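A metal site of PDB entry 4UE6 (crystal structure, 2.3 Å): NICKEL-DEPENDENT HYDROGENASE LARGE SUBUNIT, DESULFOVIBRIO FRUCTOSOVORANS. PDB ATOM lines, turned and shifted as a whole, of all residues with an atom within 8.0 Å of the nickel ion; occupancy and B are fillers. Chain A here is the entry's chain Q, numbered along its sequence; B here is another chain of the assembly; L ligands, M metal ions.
FE1 of the ligand is bound by SG of Cys 546, at 2.3 Å.
FE1 of the ligand is bound by SG of Cys 75, at 2.2 Å.
The side-chain hydroxyl (OG) of Ser 499 sits at hydrogen-bond distance from a nitrogen (N1) of the ligand (2.8 Å).
The backbone NH (N) of Arg 476 lies within hydrogen-bond range of a nitrogen (N2) of the ligand, 3.0 Å away.
A nitrogen (N1) of the ligand is in hydrogen-bond range of the backbone NH (N) of Ser 499 (3.0 Å).
A ring nitrogen (NE2) of His 79 lies within hydrogen-bond range of an oxygen (O1) of the ligand.
N2 of the ligand is in hydrogen-bond range of NH1 of Arg 476.
SG of Cys 546 sits close to NE2 of His 79 (3.2 Å).
OD of CSO 543 sits at hydrogen-bond distance from the side-chain carboxylate (OE1) of Glu 25 (2.5 Å).
The side-chain hydroxyl of Ser 499 sits at hydrogen-bond distance from N of CSO 543.
OD of CSO 543 is in hydrogen-bond range of the backbone NH (N) of Ala 545, at 3.3 Å.
The backbone NH of Val 74 lies close to the side-chain sulfur of Cys 72 (3.3 Å).
Of the 27 residues printed, 4 come within 4 Å of the nickel ion.
The nearest printed residue that does not touch the nickel ion is Arg 476 (4.3 Å).
SG of CSO 543 is bound to the nickel ion (2.2 Å).
SG of Cys 75 is bound to the nickel ion (2.2 Å).
SG of Cys 72 is bound to the nickel ion (2.2 Å).
The side-chain sulfur (SG) of Cys 546 is bound to the nickel ion (2.6 Å).
The nickel ion has four donor atoms within binding distance.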
ATOM      1  N   GLU A  25     -11.900  -6.412 -26.342  1.00  0.00           N
ATOM      2  CA  GLU A  25     -13.081  -6.391 -27.157  1.00  0.00           C
ATOM      3  C   GLU A  25     -12.983  -5.195 -28.130  1.00  0.00           C
ATOM      4  O   GLU A  25     -12.712  -4.056 -27.705  1.00  0.00           O
ATOM      5  CB  GLU A  25     -14.314  -6.297 -26.263  1.00  0.00           C
ATOM      6  CG  GLU A  25     -15.653  -6.447 -27.006  1.00  0.00           C
ATOM      7  CD  GLU A  25     -15.854  -5.407 -28.108  1.00  0.00           C
ATOM      8  OE1 GLU A  25     -15.560  -4.206 -27.844  1.00  0.00           O
ATOM      9  OE2 GLU A  25     -16.286  -5.794 -29.236  1.00  0.00           O
ATOM     10  N   GLN A  69     -28.001  -2.942 -24.951  1.00  0.00           N
ATOM     11  CA  GLN A  69     -27.298  -4.138 -24.523  1.00  0.00           C
ATOM     12  C   GLN A  69     -26.274  -4.589 -25.577  1.00  0.00           C
ATOM     13  O   GLN A  69     -25.202  -5.133 -25.226  1.00  0.00           O
ATOM     14  CB  GLN A  69     -28.216  -5.292 -24.154  1.00  0.00           C
ATOM     15  CG  GLN A  69     -27.414  -6.363 -23.408  1.00  0.00           C
ATOM     16  CD  GLN A  69     -28.224  -7.465 -22.745  1.00  0.00           C
ATOM     17  OE1 GLN A  69     -27.690  -8.179 -21.914  1.00  0.00           O
ATOM     18  NE2 GLN A  69     -29.499  -7.618 -23.133  1.00  0.00           N
ATOM     19  N   ALA A  71     -24.411  -2.796 -27.319  1.00  0.00           N
ATOM     20  CA  ALA A  71     -23.174  -2.026 -27.293  1.00  0.00           C
ATOM     21  C   ALA A  71     -22.011  -2.985 -27.073  1.00  0.00           C
ATOM     22  O   ALA A  71     -20.903  -2.755 -27.549  1.00  0.00           O
ATOM     23  CB  ALA A  71     -23.188  -0.981 -26.179  1.00  0.00           C
ATOM     24  N   CYS A  72     -22.256  -4.063 -26.347  1.00  0.00           N
ATOM     25  CA  CYS A  72     -21.187  -4.980 -26.004  1.00  0.00           C
ATOM     26  C   CYS A  72     -21.684  -6.336 -25.569  1.00  0.00           C
ATOM     27  O   CYS A  72     -22.598  -6.422 -24.771  1.00  0.00           O
ATOM     28  CB  CYS A  72     -20.320  -4.386 -24.896  1.00  0.00           C
ATOM     29  SG  CYS A  72     -18.836  -5.378 -24.594  1.00  0.00           S
ATOM     30  N   GLY A  73     -21.053  -7.395 -26.096  1.00  0.00           N
ATOM     31  CA  GLY A  73     -21.384  -8.748 -25.722  1.00  0.00           C
ATOM     32  C   GLY A  73     -20.450  -9.344 -24.683  1.00  0.00           C
ATOM     33  O   GLY A  73     -20.699 -10.427 -24.180  1.00  0.00           O
ATOM     34  N   VAL A  74     -19.357  -8.650 -24.396  1.00  0.00           N
ATOM     35  CA  VAL A  74     -18.422  -9.077 -23.359  1.00  0.00           C
ATOM     36  C   VAL A  74     -18.952  -8.593 -22.014  1.00  0.00           C
ATOM     37  O   VAL A  74     -19.210  -9.395 -21.107  1.00  0.00           O
ATOM     38  CB  VAL A  74     -16.974  -8.578 -23.626  1.00  0.00           C
ATOM     39  CG1 VAL A  74     -16.033  -9.011 -22.515  1.00  0.00           C
ATOM     40  CG2 VAL A  74     -16.480  -9.102 -24.979  1.00  0.00           C
ATOM     41  N   CYS A  75     -19.166  -7.285 -21.904  1.00  0.00           N
ATOM     42  CA  CYS A  75     -19.881  -6.770 -20.732  1.00  0.00           C
ATOM     43  C   CYS A  75     -21.361  -6.815 -21.080  1.00  0.00           C
ATOM     44  O   CYS A  75     -22.067  -5.803 -21.067  1.00  0.00           O
ATOM     45  CB  CYS A  75     -19.409  -5.382 -20.328  1.00  0.00           C
ATOM     46  SG  CYS A  75     -19.662  -4.107 -21.590  1.00  0.00           S
ATOM     47  N   THR A  76     -21.823  -8.018 -21.379  1.00  0.00           N
ATOM     48  CA  THR A  76     -23.223  -8.204 -21.641  1.00  0.00           C
ATOM     49  C   THR A  76     -23.978  -7.799 -20.372  1.00  0.00           C
ATOM     50  O   THR A  76     -23.364  -7.626 -19.321  1.00  0.00           O
ATOM     51  CB  THR A  76     -23.510  -9.655 -22.054  1.00  0.00           C
ATOM     52  OG1 THR A  76     -24.864  -9.732 -22.508  1.00  0.00           O
ATOM     53  CG2 THR A  76     -23.314 -10.594 -20.886  1.00  0.00           C
ATOM     54  N   VAL A  78     -24.789  -5.283 -18.605  1.00  0.00           N
ATOM     55  CA  VAL A  78     -24.583  -3.974 -17.940  1.00  0.00           C
ATOM     56  C   VAL A  78     -25.311  -2.808 -18.645  1.00  0.00           C
ATOM     57  O   VAL A  78     -25.877  -1.956 -17.965  1.00  0.00           O
ATOM     58  CB  VAL A  78     -23.100  -3.622 -17.719  1.00  0.00           C
ATOM     59  CG1 VAL A  78     -22.372  -4.798 -17.031  1.00  0.00           C
ATOM     60  CG2 VAL A  78     -22.405  -3.228 -19.024  1.00  0.00           C
ATOM     61  N   HIS A  79     -25.330  -2.797 -19.975  1.00  0.00           N
ATOM     62  CA  HIS A  79     -26.045  -1.741 -20.694  1.00  0.00           C
ATOM     63  C   HIS A  79     -27.556  -1.876 -20.600  1.00  0.00           C
ATOM     64  O   HIS A  79     -28.247  -0.879 -20.518  1.00  0.00           O
ATOM     65  CB  HIS A  79     -25.603  -1.646 -22.147  1.00  0.00           C
ATOM     66  CG  HIS A  79     -24.207  -1.145 -22.316  1.00  0.00           C
ATOM     67  ND1 HIS A  79     -23.862   0.183 -22.233  1.00  0.00           N
ATOM     68  CD2 HIS A  79     -23.059  -1.819 -22.578  1.00  0.00           C
ATOM     69  CE1 HIS A  79     -22.560   0.322 -22.423  1.00  0.00           C
ATOM     70  NE2 HIS A  79     -22.046  -0.877 -22.625  1.00  0.00           N
ATOM     71  N   GLN A 110     -21.883 -11.167 -13.487  1.00  0.00           N
ATOM     72  CA  GLN A 110     -21.156 -10.581 -14.621  1.00  0.00           C
ATOM     73  C   GLN A 110     -19.728 -10.211 -14.241  1.00  0.00           C
ATOM     74  O   GLN A 110     -18.818 -10.480 -15.001  1.00  0.00           O
ATOM     75  CB  GLN A 110     -21.914  -9.370 -15.186  1.00  0.00           C
ATOM     76  CG  GLN A 110     -21.231  -8.632 -16.343  1.00  0.00           C
ATOM     77  CD  GLN A 110     -20.829  -9.528 -17.521  1.00  0.00           C
ATOM     78  OE1 GLN A 110     -21.493 -10.527 -17.831  1.00  0.00           O
ATOM     79  NE2 GLN A 110     -19.744  -9.147 -18.199  1.00  0.00           N
ATOM     80  N   ASP A 114     -16.645 -11.833 -16.110  1.00  0.00           N
ATOM     81  CA  ASP A 114     -15.857 -10.850 -16.848  1.00  0.00           C
ATOM     82  C   ASP A 114     -14.412 -10.838 -16.382  1.00  0.00           C
ATOM     83  O   ASP A 114     -13.498 -10.936 -17.216  1.00  0.00           O
ATOM     84  CB  ASP A 114     -16.467  -9.436 -16.732  1.00  0.00           C
ATOM     85  CG  ASP A 114     -16.288  -8.598 -18.015  1.00  0.00           C
ATOM     86  OD1 ASP A 114     -15.211  -8.662 -18.655  1.00  0.00           O
ATOM     87  OD2 ASP A 114     -17.239  -7.857 -18.371  1.00  0.00           O
ATOM     88  N   ALA A 474     -20.015  -0.978 -14.057  1.00  0.00           N
ATOM     89  CA  ALA A 474     -19.807  -2.189 -14.802  1.00  0.00           C
ATOM     90  C   ALA A 474     -18.387  -2.754 -14.485  1.00  0.00           C
ATOM     91  O   ALA A 474     -17.585  -2.105 -13.791  1.00  0.00           O
ATOM     92  CB  ALA A 474     -19.972  -1.893 -16.272  1.00  0.00           C
ATOM     93  N   PRO A 475     -18.087  -3.963 -14.963  1.00  0.00           N
ATOM     94  CA  PRO A 475     -16.739  -4.488 -14.643  1.00  0.00           C
ATOM     95  C   PRO A 475     -15.576  -3.537 -15.005  1.00  0.00           C
ATOM     96  O   PRO A 475     -14.547  -3.524 -14.296  1.00  0.00           O
ATOM     97  CB  PRO A 475     -16.683  -5.779 -15.446  1.00  0.00           C
ATOM     98  CG  PRO A 475     -18.122  -6.226 -15.464  1.00  0.00           C
ATOM     99  CD  PRO A 475     -18.934  -4.978 -15.609  1.00  0.00           C
ATOM    100  N   ARG A 476     -15.746  -2.721 -16.047  1.00  0.00           N
ATOM    101  CA  ARG A 476     -14.690  -1.794 -16.469  1.00  0.00           C
ATOM    102  C   ARG A 476     -14.805  -0.398 -15.885  1.00  0.00           C
ATOM    103  O   ARG A 476     -13.900   0.424 -16.074  1.00  0.00           O
ATOM    104  CB  ARG A 476     -14.595  -1.752 -17.994  1.00  0.00           C
ATOM    105  CG  ARG A 476     -14.149  -3.090 -18.530  1.00  0.00           C
ATOM    106  CD  ARG A 476     -14.398  -3.272 -20.030  1.00  0.00           C
ATOM    107  NE  ARG A 476     -13.877  -4.586 -20.396  1.00  0.00           N
ATOM    108  CZ  ARG A 476     -14.544  -5.710 -20.195  1.00  0.00           C
ATOM    109  NH1 ARG A 476     -15.769  -5.665 -19.676  1.00  0.00           N
ATOM    110  NH2 ARG A 476     -13.971  -6.870 -20.509  1.00  0.00           N
ATOM    111  N   VAL A 497     -19.462   5.598 -21.386  1.00  0.00           N
ATOM    112  CA  VAL A 497     -19.103   4.246 -21.024  1.00  0.00           C
ATOM    113  C   VAL A 497     -17.680   4.220 -20.399  1.00  0.00           C
ATOM    114  O   VAL A 497     -16.858   5.073 -20.722  1.00  0.00           O
ATOM    115  CB  VAL A 497     -19.279   3.326 -22.254  1.00  0.00           C
ATOM    116  CG1 VAL A 497     -19.142   1.852 -21.893  1.00  0.00           C
ATOM    117  CG2 VAL A 497     -20.667   3.519 -22.821  1.00  0.00           C
ATOM    118  N   PRO A 498     -17.414   3.256 -19.483  1.00  0.00           N
ATOM    119  CA  PRO A 498     -16.098   3.187 -18.848  1.00  0.00           C
ATOM    120  C   PRO A 498     -14.922   3.256 -19.796  1.00  0.00           C
ATOM    121  O   PRO A 498     -13.980   3.995 -19.539  1.00  0.00           O
ATOM    122  CB  PRO A 498     -16.109   1.849 -18.111  1.00  0.00           C
ATOM    123  CG  PRO A 498     -17.469   1.246 -18.296  1.00  0.00           C
ATOM    124  CD  PRO A 498     -18.367   2.342 -18.826  1.00  0.00           C
ATOM    125  N   SER A 499     -14.964   2.493 -20.886  1.00  0.00           N
ATOM    126  CA  SER A 499     -13.855   2.526 -21.843  1.00  0.00           C
ATOM    127  C   SER A 499     -13.761   3.867 -22.550  1.00  0.00           C
ATOM    128  O   SER A 499     -12.669   4.245 -22.977  1.00  0.00           O
ATOM    129  CB  SER A 499     -13.903   1.370 -22.857  1.00  0.00           C
ATOM    130  OG  SER A 499     -13.594   0.146 -22.192  1.00  0.00           O
ATOM    131  N   ASP A 541      -8.422  -3.195 -19.437  1.00  0.00           N
ATOM    132  CA  ASP A 541      -9.505  -4.067 -19.920  1.00  0.00           C
ATOM    133  C   ASP A 541     -10.364  -3.331 -21.007  1.00  0.00           C
ATOM    134  O   ASP A 541     -11.580  -3.125 -20.843  1.00  0.00           O
ATOM    135  CB  ASP A 541     -10.332  -4.507 -18.707  1.00  0.00           C
ATOM    136  CG  ASP A 541     -11.318  -5.613 -19.034  1.00  0.00           C
ATOM    137  OD1 ASP A 541     -11.411  -6.125 -20.200  1.00  0.00           O
ATOM    138  OD2 ASP A 541     -12.045  -5.979 -18.079  1.00  0.00           O
ATOM    139  N   PRO A 542      -9.721  -2.916 -22.107  1.00  0.00           N
ATOM    140  CA  PRO A 542     -10.412  -2.088 -23.085  1.00  0.00           C
ATOM    141  C   PRO A 542     -11.600  -2.807 -23.733  1.00  0.00           C
ATOM    142  O   PRO A 542     -11.484  -3.987 -24.098  1.00  0.00           O
ATOM    143  CB  PRO A 542      -9.333  -1.825 -24.153  1.00  0.00           C
ATOM    144  CG  PRO A 542      -8.044  -2.095 -23.446  1.00  0.00           C
ATOM    145  CD  PRO A 542      -8.344  -3.212 -22.511  1.00  0.00           C
ATOM    146  N   CSO A 543     -12.697  -2.075 -23.906  1.00  0.00           N
ATOM    147  CA  CSO A 543     -13.862  -2.506 -24.656  1.00  0.00           C
ATOM    148  CB  CSO A 543     -14.967  -2.784 -23.650  1.00  0.00           C
ATOM    149  SG  CSO A 543     -16.259  -3.801 -24.311  1.00  0.00           S
ATOM    150  C   CSO A 543     -14.224  -1.396 -25.625  1.00  0.00           C
ATOM    151  O   CSO A 543     -14.821  -0.381 -25.252  1.00  0.00           O
ATOM    152  OD  CSO A 543     -16.785  -3.313 -25.892  1.00  0.00           O
ATOM    153  N   ILE A 544     -13.873  -1.557 -26.905  1.00  0.00           N
ATOM    154  CA  ILE A 544     -14.001  -0.455 -27.861  1.00  0.00           C
ATOM    155  C   ILE A 544     -15.430  -0.349 -28.394  1.00  0.00           C
ATOM    156  O   ILE A 544     -15.880   0.739 -28.710  1.00  0.00           O
ATOM    157  CB  ILE A 544     -12.996  -0.565 -29.028  1.00  0.00           C
ATOM    158  CG1 ILE A 544     -11.591  -0.822 -28.504  1.00  0.00           C
ATOM    159  CG2 ILE A 544     -13.022   0.657 -29.925  1.00  0.00           C
ATOM    160  CD1 ILE A 544     -11.102   0.147 -27.446  1.00  0.00           C
ATOM    161  N   ALA A 545     -16.121  -1.488 -28.504  1.00  0.00           N
ATOM    162  CA  ALA A 545     -17.533  -1.486 -28.886  1.00  0.00           C
ATOM    163  C   ALA A 545     -18.319  -0.681 -27.827  1.00  0.00           C
ATOM    164  O   ALA A 545     -19.183   0.130 -28.150  1.00  0.00           O
ATOM    165  CB  ALA A 545     -18.069  -2.916 -29.034  1.00  0.00           C
ATOM    166  N   CYS A 546     -17.974  -0.920 -26.562  1.00  0.00           N
ATOM    167  CA  CYS A 546     -18.492  -0.128 -25.452  1.00  0.00           C
ATOM    168  C   CYS A 546     -18.137   1.363 -25.547  1.00  0.00           C
ATOM    169  O   CYS A 546     -19.014   2.229 -25.452  1.00  0.00           O
ATOM    170  CB  CYS A 546     -17.936  -0.663 -24.129  1.00  0.00           C
ATOM    171  SG  CYS A 546     -19.063  -1.751 -23.264  1.00  0.00           S
ATOM    172  N   GLY A 547     -16.845   1.653 -25.716  1.00  0.00           N
ATOM    173  CA  GLY A 547     -16.344   3.012 -25.699  1.00  0.00           C
ATOM    174  C   GLY A 547     -16.971   3.877 -26.766  1.00  0.00           C
ATOM    175  O   GLY A 547     -17.313   5.015 -26.502  1.00  0.00           O
ATOM    176  N   CYS B  17     -20.405  -6.711 -31.548  1.00  0.00           N
ATOM    177  CA  CYS B  17     -20.329  -6.420 -30.118  1.00  0.00           C
ATOM    178  C   CYS B  17     -19.492  -7.486 -29.377  1.00  0.00           C
ATOM    179  O   CYS B  17     -19.230  -7.363 -28.186  1.00  0.00           O
ATOM    180  CB  CYS B  17     -21.727  -6.329 -29.509  1.00  0.00           C
ATOM    181  SG  CYS B  17     -22.487  -7.918 -29.096  1.00  0.00           S
ATOM    182  N   THR B  18     -19.086  -8.503 -30.130  1.00  0.00           N
ATOM    183  CA  THR B  18     -18.302  -9.647 -29.622  1.00  0.00           C
ATOM    184  C   THR B  18     -19.174 -10.618 -28.814  1.00  0.00           C
ATOM    185  O   THR B  18     -18.681 -11.594 -28.263  1.00  0.00           O
ATOM    186  CB  THR B  18     -17.028  -9.181 -28.853  1.00  0.00           C
ATOM    187  OG1 THR B  18     -16.282  -8.297 -29.691  1.00  0.00           O
ATOM    188  CG2 THR B  18     -16.126 -10.355 -28.452  1.00  0.00           C
HETATM  189 FE1  LIG L   1     -18.366  -2.343 -21.126  1.00  0.00          FE
HETATM  190  C1  LIG L   1     -16.987  -1.033 -21.185  1.00  0.00           C
HETATM  191  N1  LIG L   1     -16.169  -0.200 -21.232  1.00  0.00           N
HETATM  192  C2  LIG L   1     -17.897  -2.922 -19.375  1.00  0.00           C
HETATM  193  N2  LIG L   1     -17.686  -3.254 -18.290  1.00  0.00           N
HETATM  194  C3  LIG L   1     -19.418  -1.213 -20.354  1.00  0.00           C
HETATM  195  O1  LIG L   1     -20.124  -0.488 -19.833  1.00  0.00           O
HETATM  196 NI    NI M   1     -17.941  -4.086 -22.985  1.00  0.00          NI
